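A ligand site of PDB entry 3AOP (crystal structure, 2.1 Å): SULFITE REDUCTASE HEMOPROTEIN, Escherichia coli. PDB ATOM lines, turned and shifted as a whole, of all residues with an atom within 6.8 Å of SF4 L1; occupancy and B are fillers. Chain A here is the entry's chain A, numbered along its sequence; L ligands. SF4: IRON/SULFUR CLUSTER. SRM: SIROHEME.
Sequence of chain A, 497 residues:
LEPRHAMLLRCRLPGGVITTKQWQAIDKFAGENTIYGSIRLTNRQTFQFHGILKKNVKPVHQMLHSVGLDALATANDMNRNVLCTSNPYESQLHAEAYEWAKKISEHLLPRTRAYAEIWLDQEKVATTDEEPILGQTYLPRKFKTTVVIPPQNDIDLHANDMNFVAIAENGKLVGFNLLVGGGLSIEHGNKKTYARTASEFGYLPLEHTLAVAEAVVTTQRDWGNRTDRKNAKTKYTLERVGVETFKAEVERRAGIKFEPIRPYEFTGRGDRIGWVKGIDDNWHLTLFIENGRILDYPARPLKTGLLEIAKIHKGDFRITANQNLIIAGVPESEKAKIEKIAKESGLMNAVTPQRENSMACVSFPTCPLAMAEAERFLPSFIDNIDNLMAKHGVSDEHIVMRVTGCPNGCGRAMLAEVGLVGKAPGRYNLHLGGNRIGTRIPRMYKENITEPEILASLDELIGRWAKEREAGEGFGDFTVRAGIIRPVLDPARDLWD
S2 of SF4 L1 lies close to OG1 of Thr 404 (3.3 Å). The side-chain amide nitrogen (ND2) of Asn 408 lies close to a sulfur (S1) of SF4 L1 (3.7 Å). The backbone NH of Val 362 sits at hydrogen-bond distance from an oxygen (O3B) of SRM L2 (3.0 Å). N of Cys 410 sits close to S2 of SF4 L1, at 3.4 Å. N of Cys 367 is in hydrogen-bond range of O1A of SRM L2 (3.4 Å). An iron atom (FE) of SRM L2 is bound by the side-chain sulfur of Cys 410. S2 of SF4 L1 lies close to N of Gly 409 (3.8 Å). An iron atom (FE3) of SF4 L1 is bound by the side-chain sulfur (SG) of Cys 406 (2.2 Å). SG of Cys 361 binds FE1 of SF4 L1 (2.2 Å). SG of Cys 410 is bound to FE4 of SF4 L1 (2.2 Å). The side-chain sulfur (SG) of Cys 367 is bound to an iron atom (FE2) of SF4 L1, at 2.2 Å. N of Ser 363 sits close to S3 of SF4 L1.
The side-chain sulfur (SG) of Cys 406 sits close to the side-chain amide nitrogen (ND2) of Asn 408 (3.5 Å). The backbone NH of Gly 411 sits at hydrogen-bond distance from the side-chain hydroxyl of Thr 404, 3.0 Å away. The side-chain sulfur of Cys 361 sits close to the backbone NH of Gly 405 (3.2 Å). SG of Cys 361 sits close to N of Ser 363 (3.7 Å). O of Gly 405 lies within hydrogen-bond range of N of Ala 372, at 3.1 Å. The side-chain hydroxyl (OG1) of Thr 404 sits at hydrogen-bond distance from the backbone NH (N) of Cys 410, 3.2 Å away. The backbone carbonyl oxygen (O) of Val 403 is in hydrogen-bond range of the backbone NH (N) of Cys 361. The side-chain sulfur of Cys 406 lies close to the backbone carbonyl oxygen of Leu 369.
Leu 369 touches SF4 L1 (CB to S1, 3.9 Å). Ala 370 touches SF4 L1 (CA to S4, 3.5 Å). Gly 405 touches SF4 L1. Hydrophobic or aromatic side chains that line SF4 L1: Leu 369 and Ala 370. Within 4 Å of SF4 L1: Cys 361, Ser 363, Cys 367, Leu 369, Ala 370, Thr 404, Gly 405, Cys 406, Asn 408, Gly 409 and Cys 410.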
ATOM      1  N   ALA A 360     -13.919 -14.853  34.502  1.00  0.00           N
ATOM      2  CA  ALA A 360     -14.452 -16.202  34.444  1.00  0.00           C
ATOM      3  C   ALA A 360     -14.819 -16.508  32.996  1.00  0.00           C
ATOM      4  O   ALA A 360     -14.960 -15.582  32.180  1.00  0.00           O
ATOM      5  CB  ALA A 360     -15.700 -16.319  35.339  1.00  0.00           C
ATOM      6  N   CYS A 361     -14.849 -17.789  32.651  1.00  0.00           N
ATOM      7  CA  CYS A 361     -15.240 -18.225  31.306  1.00  0.00           C
ATOM      8  C   CYS A 361     -16.785 -18.363  31.253  1.00  0.00           C
ATOM      9  O   CYS A 361     -17.475 -18.246  32.286  1.00  0.00           O
ATOM     10  CB  CYS A 361     -14.601 -19.570  30.961  1.00  0.00           C
ATOM     11  SG  CYS A 361     -15.366 -20.965  31.848  1.00  0.00           S
ATOM     12  N   VAL A 362     -17.323 -18.584  30.050  1.00  0.00           N
ATOM     13  CA  VAL A 362     -18.760 -18.745  29.871  1.00  0.00           C
ATOM     14  C   VAL A 362     -19.361 -19.877  30.708  1.00  0.00           C
ATOM     15  O   VAL A 362     -20.251 -19.648  31.528  1.00  0.00           O
ATOM     16  CB  VAL A 362     -19.122 -18.946  28.396  1.00  0.00           C
ATOM     17  CG1 VAL A 362     -20.578 -19.249  28.257  1.00  0.00           C
ATOM     18  CG2 VAL A 362     -18.794 -17.682  27.604  1.00  0.00           C
ATOM     19  N   SER A 363     -18.867 -21.103  30.518  1.00  0.00           N
ATOM     20  CA  SER A 363     -19.360 -22.270  31.274  1.00  0.00           C
ATOM     21  C   SER A 363     -20.886 -22.475  31.055  1.00  0.00           C
ATOM     22  O   SER A 363     -21.382 -22.227  29.950  1.00  0.00           O
ATOM     23  CB  SER A 363     -19.059 -22.102  32.766  1.00  0.00           C
ATOM     24  OG  SER A 363     -19.297 -23.310  33.459  1.00  0.00           O
ATOM     25  N   PHE A 364     -21.606 -22.959  32.072  1.00  0.00           N
ATOM     26  CA  PHE A 364     -23.048 -23.172  31.968  1.00  0.00           C
ATOM     27  C   PHE A 364     -23.684 -21.808  31.753  1.00  0.00           C
ATOM     28  O   PHE A 364     -23.204 -20.828  32.315  1.00  0.00           O
ATOM     29  CB  PHE A 364     -23.611 -23.767  33.247  1.00  0.00           C
ATOM     30  CG  PHE A 364     -23.054 -25.087  33.623  1.00  0.00           C
ATOM     31  CD1 PHE A 364     -23.310 -26.200  32.845  1.00  0.00           C
ATOM     32  CD2 PHE A 364     -22.278 -25.228  34.765  1.00  0.00           C
ATOM     33  CE1 PHE A 364     -22.803 -27.451  33.205  1.00  0.00           C
ATOM     34  CE2 PHE A 364     -21.764 -26.460  35.125  1.00  0.00           C
ATOM     35  CZ  PHE A 364     -22.033 -27.569  34.343  1.00  0.00           C
ATOM     36  N   CYS A 367     -21.995 -23.826  27.598  1.00  0.00           N
ATOM     37  CA  CYS A 367     -20.829 -24.662  27.301  1.00  0.00           C
ATOM     38  C   CYS A 367     -21.070 -26.147  27.574  1.00  0.00           C
ATOM     39  O   CYS A 367     -21.292 -26.547  28.710  1.00  0.00           O
ATOM     40  CB  CYS A 367     -19.597 -24.211  28.070  1.00  0.00           C
ATOM     41  SG  CYS A 367     -18.126 -25.113  27.513  1.00  0.00           S
ATOM     42  N   PRO A 368     -20.953 -26.980  26.546  1.00  0.00           N
ATOM     43  CA  PRO A 368     -21.168 -28.419  26.720  1.00  0.00           C
ATOM     44  C   PRO A 368     -20.058 -29.160  27.473  1.00  0.00           C
ATOM     45  O   PRO A 368     -20.225 -30.313  27.867  1.00  0.00           O
ATOM     46  CB  PRO A 368     -21.289 -28.901  25.281  1.00  0.00           C
ATOM     47  CG  PRO A 368     -20.369 -27.961  24.537  1.00  0.00           C
ATOM     48  CD  PRO A 368     -20.729 -26.629  25.129  1.00  0.00           C
ATOM     49  N   LEU A 369     -18.934 -28.484  27.694  1.00  0.00           N
ATOM     50  CA  LEU A 369     -17.818 -29.111  28.362  1.00  0.00           C
ATOM     51  C   LEU A 369     -17.718 -28.674  29.792  1.00  0.00           C
ATOM     52  O   LEU A 369     -16.867 -29.149  30.527  1.00  0.00           O
ATOM     53  CB  LEU A 369     -16.512 -28.763  27.634  1.00  0.00           C
ATOM     54  CG  LEU A 369     -16.538 -28.981  26.114  1.00  0.00           C
ATOM     55  CD1 LEU A 369     -15.201 -28.615  25.501  1.00  0.00           C
ATOM     56  CD2 LEU A 369     -16.877 -30.444  25.803  1.00  0.00           C
ATOM     57  N   ALA A 370     -18.639 -27.816  30.210  1.00  0.00           N
ATOM     58  CA  ALA A 370     -18.619 -27.287  31.565  1.00  0.00           C
ATOM     59  C   ALA A 370     -18.728 -28.335  32.664  1.00  0.00           C
ATOM     60  O   ALA A 370     -19.499 -29.289  32.556  1.00  0.00           O
ATOM     61  CB  ALA A 370     -19.725 -26.257  31.704  1.00  0.00           C
ATOM     62  N   MET A 371     -17.914 -28.182  33.716  1.00  0.00           N
ATOM     63  CA  MET A 371     -17.960 -29.094  34.866  1.00  0.00           C
ATOM     64  C   MET A 371     -18.538 -28.332  36.075  1.00  0.00           C
ATOM     65  O   MET A 371     -19.284 -28.888  36.858  1.00  0.00           O
ATOM     66  CB  MET A 371     -16.574 -29.635  35.184  1.00  0.00           C
ATOM     67  CG  MET A 371     -16.028 -30.631  34.156  1.00  0.00           C
ATOM     68  SD  MET A 371     -14.277 -30.989  34.491  1.00  0.00           S
ATOM     69  CE  MET A 371     -13.837 -32.135  33.163  1.00  0.00           C
ATOM     70  N   ALA A 372     -18.199 -27.056  36.194  1.00  0.00           N
ATOM     71  CA  ALA A 372     -18.693 -26.225  37.287  1.00  0.00           C
ATOM     72  C   ALA A 372     -19.001 -24.847  36.733  1.00  0.00           C
ATOM     73  O   ALA A 372     -18.535 -24.499  35.657  1.00  0.00           O
ATOM     74  CB  ALA A 372     -17.652 -26.138  38.382  1.00  0.00           C
ATOM     75  N   ALA A 374     -18.992 -20.793  36.194  1.00  0.00           N
ATOM     76  CA  ALA A 374     -17.893 -19.841  36.182  1.00  0.00           C
ATOM     77  C   ALA A 374     -18.488 -18.459  36.041  1.00  0.00           C
ATOM     78  O   ALA A 374     -18.590 -17.726  37.027  1.00  0.00           O
ATOM     79  CB  ALA A 374     -16.947 -20.147  35.067  1.00  0.00           C
ATOM     80  N   VAL A 403     -11.742 -17.822  37.375  1.00  0.00           N
ATOM     81  CA  VAL A 403     -12.470 -19.057  37.513  1.00  0.00           C
ATOM     82  C   VAL A 403     -12.702 -19.620  36.132  1.00  0.00           C
ATOM     83  O   VAL A 403     -13.190 -18.935  35.243  1.00  0.00           O
ATOM     84  CB  VAL A 403     -13.850 -18.809  38.173  1.00  0.00           C
ATOM     85  CG1 VAL A 403     -14.589 -20.137  38.379  1.00  0.00           C
ATOM     86  CG2 VAL A 403     -13.671 -18.080  39.502  1.00  0.00           C
ATOM     87  N   THR A 404     -12.317 -20.873  35.941  1.00  0.00           N
ATOM     88  CA  THR A 404     -12.499 -21.527  34.665  1.00  0.00           C
ATOM     89  C   THR A 404     -13.391 -22.743  34.959  1.00  0.00           C
ATOM     90  O   THR A 404     -13.219 -23.429  35.971  1.00  0.00           O
ATOM     91  CB  THR A 404     -11.088 -21.838  34.008  1.00  0.00           C
ATOM     92  OG1 THR A 404     -11.251 -22.012  32.599  1.00  0.00           O
ATOM     93  CG2 THR A 404     -10.429 -23.080  34.599  1.00  0.00           C
ATOM     94  N   GLY A 405     -14.410 -22.947  34.131  1.00  0.00           N
ATOM     95  CA  GLY A 405     -15.389 -24.016  34.331  1.00  0.00           C
ATOM     96  C   GLY A 405     -14.940 -25.449  34.194  1.00  0.00           C
ATOM     97  O   GLY A 405     -15.610 -26.363  34.682  1.00  0.00           O
ATOM     98  N   CYS A 406     -13.828 -25.661  33.520  1.00  0.00           N
ATOM     99  CA  CYS A 406     -13.267 -26.983  33.329  1.00  0.00           C
ATOM    100  C   CYS A 406     -11.803 -26.727  33.007  1.00  0.00           C
ATOM    101  O   CYS A 406     -11.426 -25.582  32.714  1.00  0.00           O
ATOM    102  CB  CYS A 406     -14.006 -27.760  32.208  1.00  0.00           C
ATOM    103  SG  CYS A 406     -13.644 -27.302  30.476  1.00  0.00           S
ATOM    104  N   PRO A 407     -10.953 -27.760  33.063  1.00  0.00           N
ATOM    105  CA  PRO A 407      -9.511 -27.645  32.795  1.00  0.00           C
ATOM    106  C   PRO A 407      -9.059 -27.129  31.423  1.00  0.00           C
ATOM    107  O   PRO A 407      -7.876 -26.834  31.236  1.00  0.00           O
ATOM    108  CB  PRO A 407      -8.999 -29.044  33.122  1.00  0.00           C
ATOM    109  CG  PRO A 407     -10.145 -29.920  32.719  1.00  0.00           C
ATOM    110  CD  PRO A 407     -11.327 -29.168  33.300  1.00  0.00           C
ATOM    111  N   ASN A 408      -9.978 -27.027  30.461  1.00  0.00           N
ATOM    112  CA  ASN A 408      -9.631 -26.497  29.128  1.00  0.00           C
ATOM    113  C   ASN A 408      -9.040 -25.085  29.341  1.00  0.00           C
ATOM    114  O   ASN A 408      -8.277 -24.597  28.522  1.00  0.00           O
ATOM    115  CB  ASN A 408     -10.863 -26.460  28.192  1.00  0.00           C
ATOM    116  CG  ASN A 408     -11.176 -27.853  27.599  1.00  0.00           C
ATOM    117  OD1 ASN A 408     -10.287 -28.694  27.449  1.00  0.00           O
ATOM    118  ND2 ASN A 408     -12.432 -28.103  27.286  1.00  0.00           N
ATOM    119  N   GLY A 409      -9.406 -24.455  30.447  1.00  0.00           N
ATOM    120  CA  GLY A 409      -8.851 -23.170  30.819  1.00  0.00           C
ATOM    121  C   GLY A 409      -9.182 -21.868  30.133  1.00  0.00           C
ATOM    122  O   GLY A 409      -8.390 -20.931  30.225  1.00  0.00           O
ATOM    123  N   CYS A 410     -10.345 -21.764  29.500  1.00  0.00           N
ATOM    124  CA  CYS A 410     -10.750 -20.542  28.817  1.00  0.00           C
ATOM    125  C   CYS A 410     -10.740 -19.285  29.697  1.00  0.00           C
ATOM    126  O   CYS A 410     -10.506 -18.205  29.213  1.00  0.00           O
ATOM    127  CB  CYS A 410     -12.130 -20.704  28.229  1.00  0.00           C
ATOM    128  SG  CYS A 410     -12.228 -22.236  27.273  1.00  0.00           S
ATOM    129  N   GLY A 411     -10.996 -19.444  30.984  1.00  0.00           N
ATOM    130  CA  GLY A 411     -11.009 -18.306  31.888  1.00  0.00           C
ATOM    131  C   GLY A 411      -9.612 -17.841  32.294  1.00  0.00           C
ATOM    132  O   GLY A 411      -9.492 -16.893  33.058  1.00  0.00           O
HETATM  133 FE1  SF4 L   1     -15.253 -22.708  30.502  1.00  0.00          FE
HETATM  134 FE2  SF4 L   1     -16.448 -24.323  28.670  1.00  0.00          FE
HETATM  135 FE3  SF4 L   1     -14.471 -25.342  29.991  1.00  0.00          FE
HETATM  136 FE4  SF4 L   1     -13.963 -23.236  28.274  1.00  0.00          FE
HETATM  137  S1  SF4 L   1     -14.701 -25.269  27.781  1.00  0.00           S
HETATM  138  S2  SF4 L   1     -13.074 -23.590  30.386  1.00  0.00           S
HETATM  139  S3  SF4 L   1     -15.895 -22.027  28.516  1.00  0.00           S
HETATM  140  S4  SF4 L   1     -16.443 -24.658  30.873  1.00  0.00           S
HETATM  141 FE   SRM L   2     -12.106 -21.577  24.665  1.00  0.00          FE
HETATM  142  CHA SRM L   2     -13.405 -24.598  23.853  1.00  0.00           C
HETATM  143  CHB SRM L   2     -15.275 -20.405  25.284  1.00  0.00           C
HETATM  144  CHC SRM L   2     -10.805 -18.587  25.422  1.00  0.00           C
HETATM  145  CHD SRM L   2      -9.036 -23.005  25.516  1.00  0.00           C
HETATM  146  NA  SRM L   2     -14.018 -22.308  24.512  1.00  0.00           N
HETATM  147  C1A SRM L   2     -14.307 -23.582  23.953  1.00  0.00           C
HETATM  148  C2A SRM L   2     -15.803 -23.669  23.683  1.00  0.00           C
HETATM  149  CMA SRM L   2     -16.002 -23.155  22.181  1.00  0.00           C
HETATM  150  CDA SRM L   2     -16.457 -25.037  23.926  1.00  0.00           C
HETATM  151  CEA SRM L   2     -16.527 -26.048  22.792  1.00  0.00           C
HETATM  152  O3A SRM L   2     -15.461 -26.489  22.296  1.00  0.00           O
HETATM  153  O4A SRM L   2     -17.646 -26.416  22.387  1.00  0.00           O
HETATM  154  C3A SRM L   2     -16.309 -22.708  24.752  1.00  0.00           C
HETATM  155  CAA SRM L   2     -17.600 -22.080  24.290  1.00  0.00           C
HETATM  156  CBA SRM L   2     -18.427 -21.763  25.526  1.00  0.00           C
HETATM  157  CCA SRM L   2     -19.688 -20.948  25.228  1.00  0.00           C
HETATM  158  O1A SRM L   2     -20.798 -21.426  25.522  1.00  0.00           O
HETATM  159  O2A SRM L   2     -19.573 -19.817  24.707  1.00  0.00           O
HETATM  160  C4A SRM L   2     -15.187 -21.714  24.888  1.00  0.00           C
HETATM  161  NB  SRM L   2     -12.904 -19.811  25.109  1.00  0.00           N
HETATM  162  C1B SRM L   2     -14.215 -19.516  25.375  1.00  0.00           C
HETATM  163  C2B SRM L   2     -14.330 -18.061  25.712  1.00  0.00           C
HETATM  164  CMB SRM L   2     -15.644 -17.496  25.074  1.00  0.00           C
HETATM  165  CDB SRM L   2     -14.329 -17.857  27.314  1.00  0.00           C
HETATM  166  CEB SRM L   2     -14.767 -16.519  27.860  1.00  0.00           C
HETATM  167  O3B SRM L   2     -15.609 -16.487  28.775  1.00  0.00           O
HETATM  168  O4B SRM L   2     -14.280 -15.471  27.365  1.00  0.00           O
HETATM  169  C3B SRM L   2     -13.097 -17.531  24.971  1.00  0.00           C
HETATM  170  CAB SRM L   2     -13.395 -17.489  23.474  1.00  0.00           C
HETATM  171  CBB SRM L   2     -12.217 -16.682  22.987  1.00  0.00           C
HETATM  172  CCB SRM L   2     -12.300 -16.386  21.524  1.00  0.00           C
HETATM  173  O1B SRM L   2     -12.926 -15.370  21.172  1.00  0.00           O
HETATM  174  O2B SRM L   2     -11.752 -17.166  20.717  1.00  0.00           O
HETATM  175  C4B SRM L   2     -12.167 -18.689  25.271  1.00  0.00           C
HETATM  176  NC  SRM L   2     -10.222 -20.878  25.367  1.00  0.00           N
HETATM  177  C1C SRM L   2      -9.893 -19.609  25.491  1.00  0.00           C
HETATM  178  C2C SRM L   2      -8.634 -19.547  26.268  1.00  0.00           C
HETATM  179  CDC SRM L   2      -7.920 -18.294  26.635  1.00  0.00           C
HETATM  180  CEC SRM L   2      -7.338 -17.456  25.513  1.00  0.00           C
HETATM  181  O3C SRM L   2      -7.306 -17.910  24.355  1.00  0.00           O
HETATM  182  O4C SRM L   2      -6.894 -16.323  25.788  1.00  0.00           O
HETATM  183  C3C SRM L   2      -8.112 -20.776  26.296  1.00  0.00           C
HETATM  184  CAC SRM L   2      -6.871 -21.118  27.034  1.00  0.00           C
HETATM  185  CBC SRM L   2      -5.512 -21.000  26.368  1.00  0.00           C
HETATM  186  CCC SRM L   2      -5.205 -22.161  25.455  1.00  0.00           C
HETATM  187  O1C SRM L   2      -5.804 -22.227  24.367  1.00  0.00           O
HETATM  188  O2C SRM L   2      -4.394 -23.028  25.826  1.00  0.00           O
HETATM  189  C4C SRM L   2      -9.101 -21.637  25.688  1.00  0.00           C
HETATM  190  ND  SRM L   2     -11.344 -23.453  24.606  1.00  0.00           N
HETATM  191  C1D SRM L   2     -10.043 -23.831  24.997  1.00  0.00           C
HETATM  192  C2D SRM L   2      -9.995 -25.298  24.790  1.00  0.00           C
HETATM  193  CAD SRM L   2      -8.824 -26.220  25.060  1.00  0.00           C
HETATM  194  CBD SRM L   2      -7.856 -26.089  23.895  1.00  0.00           C
HETATM  195  CCD SRM L   2      -6.673 -27.023  23.979  1.00  0.00           C
HETATM  196  O1D SRM L   2      -5.641 -26.754  23.323  1.00  0.00           O
HETATM  197  O2D SRM L   2      -6.768 -28.047  24.687  1.00  0.00           O
HETATM  198  C3D SRM L   2     -11.215 -25.683  24.275  1.00  0.00           C
HETATM  199  CDD SRM L   2     -11.749 -27.069  23.870  1.00  0.00           C
HETATM  200  CED SRM L   2     -11.148 -27.679  22.621  1.00  0.00           C
HETATM  201  O3D SRM L   2     -10.964 -26.964  21.632  1.00  0.00           O
HETATM  202  O4D SRM L   2     -10.860 -28.882  22.636  1.00  0.00           O
HETATM  203  C4D SRM L   2     -12.090 -24.536  24.199  1.00  0.00           C
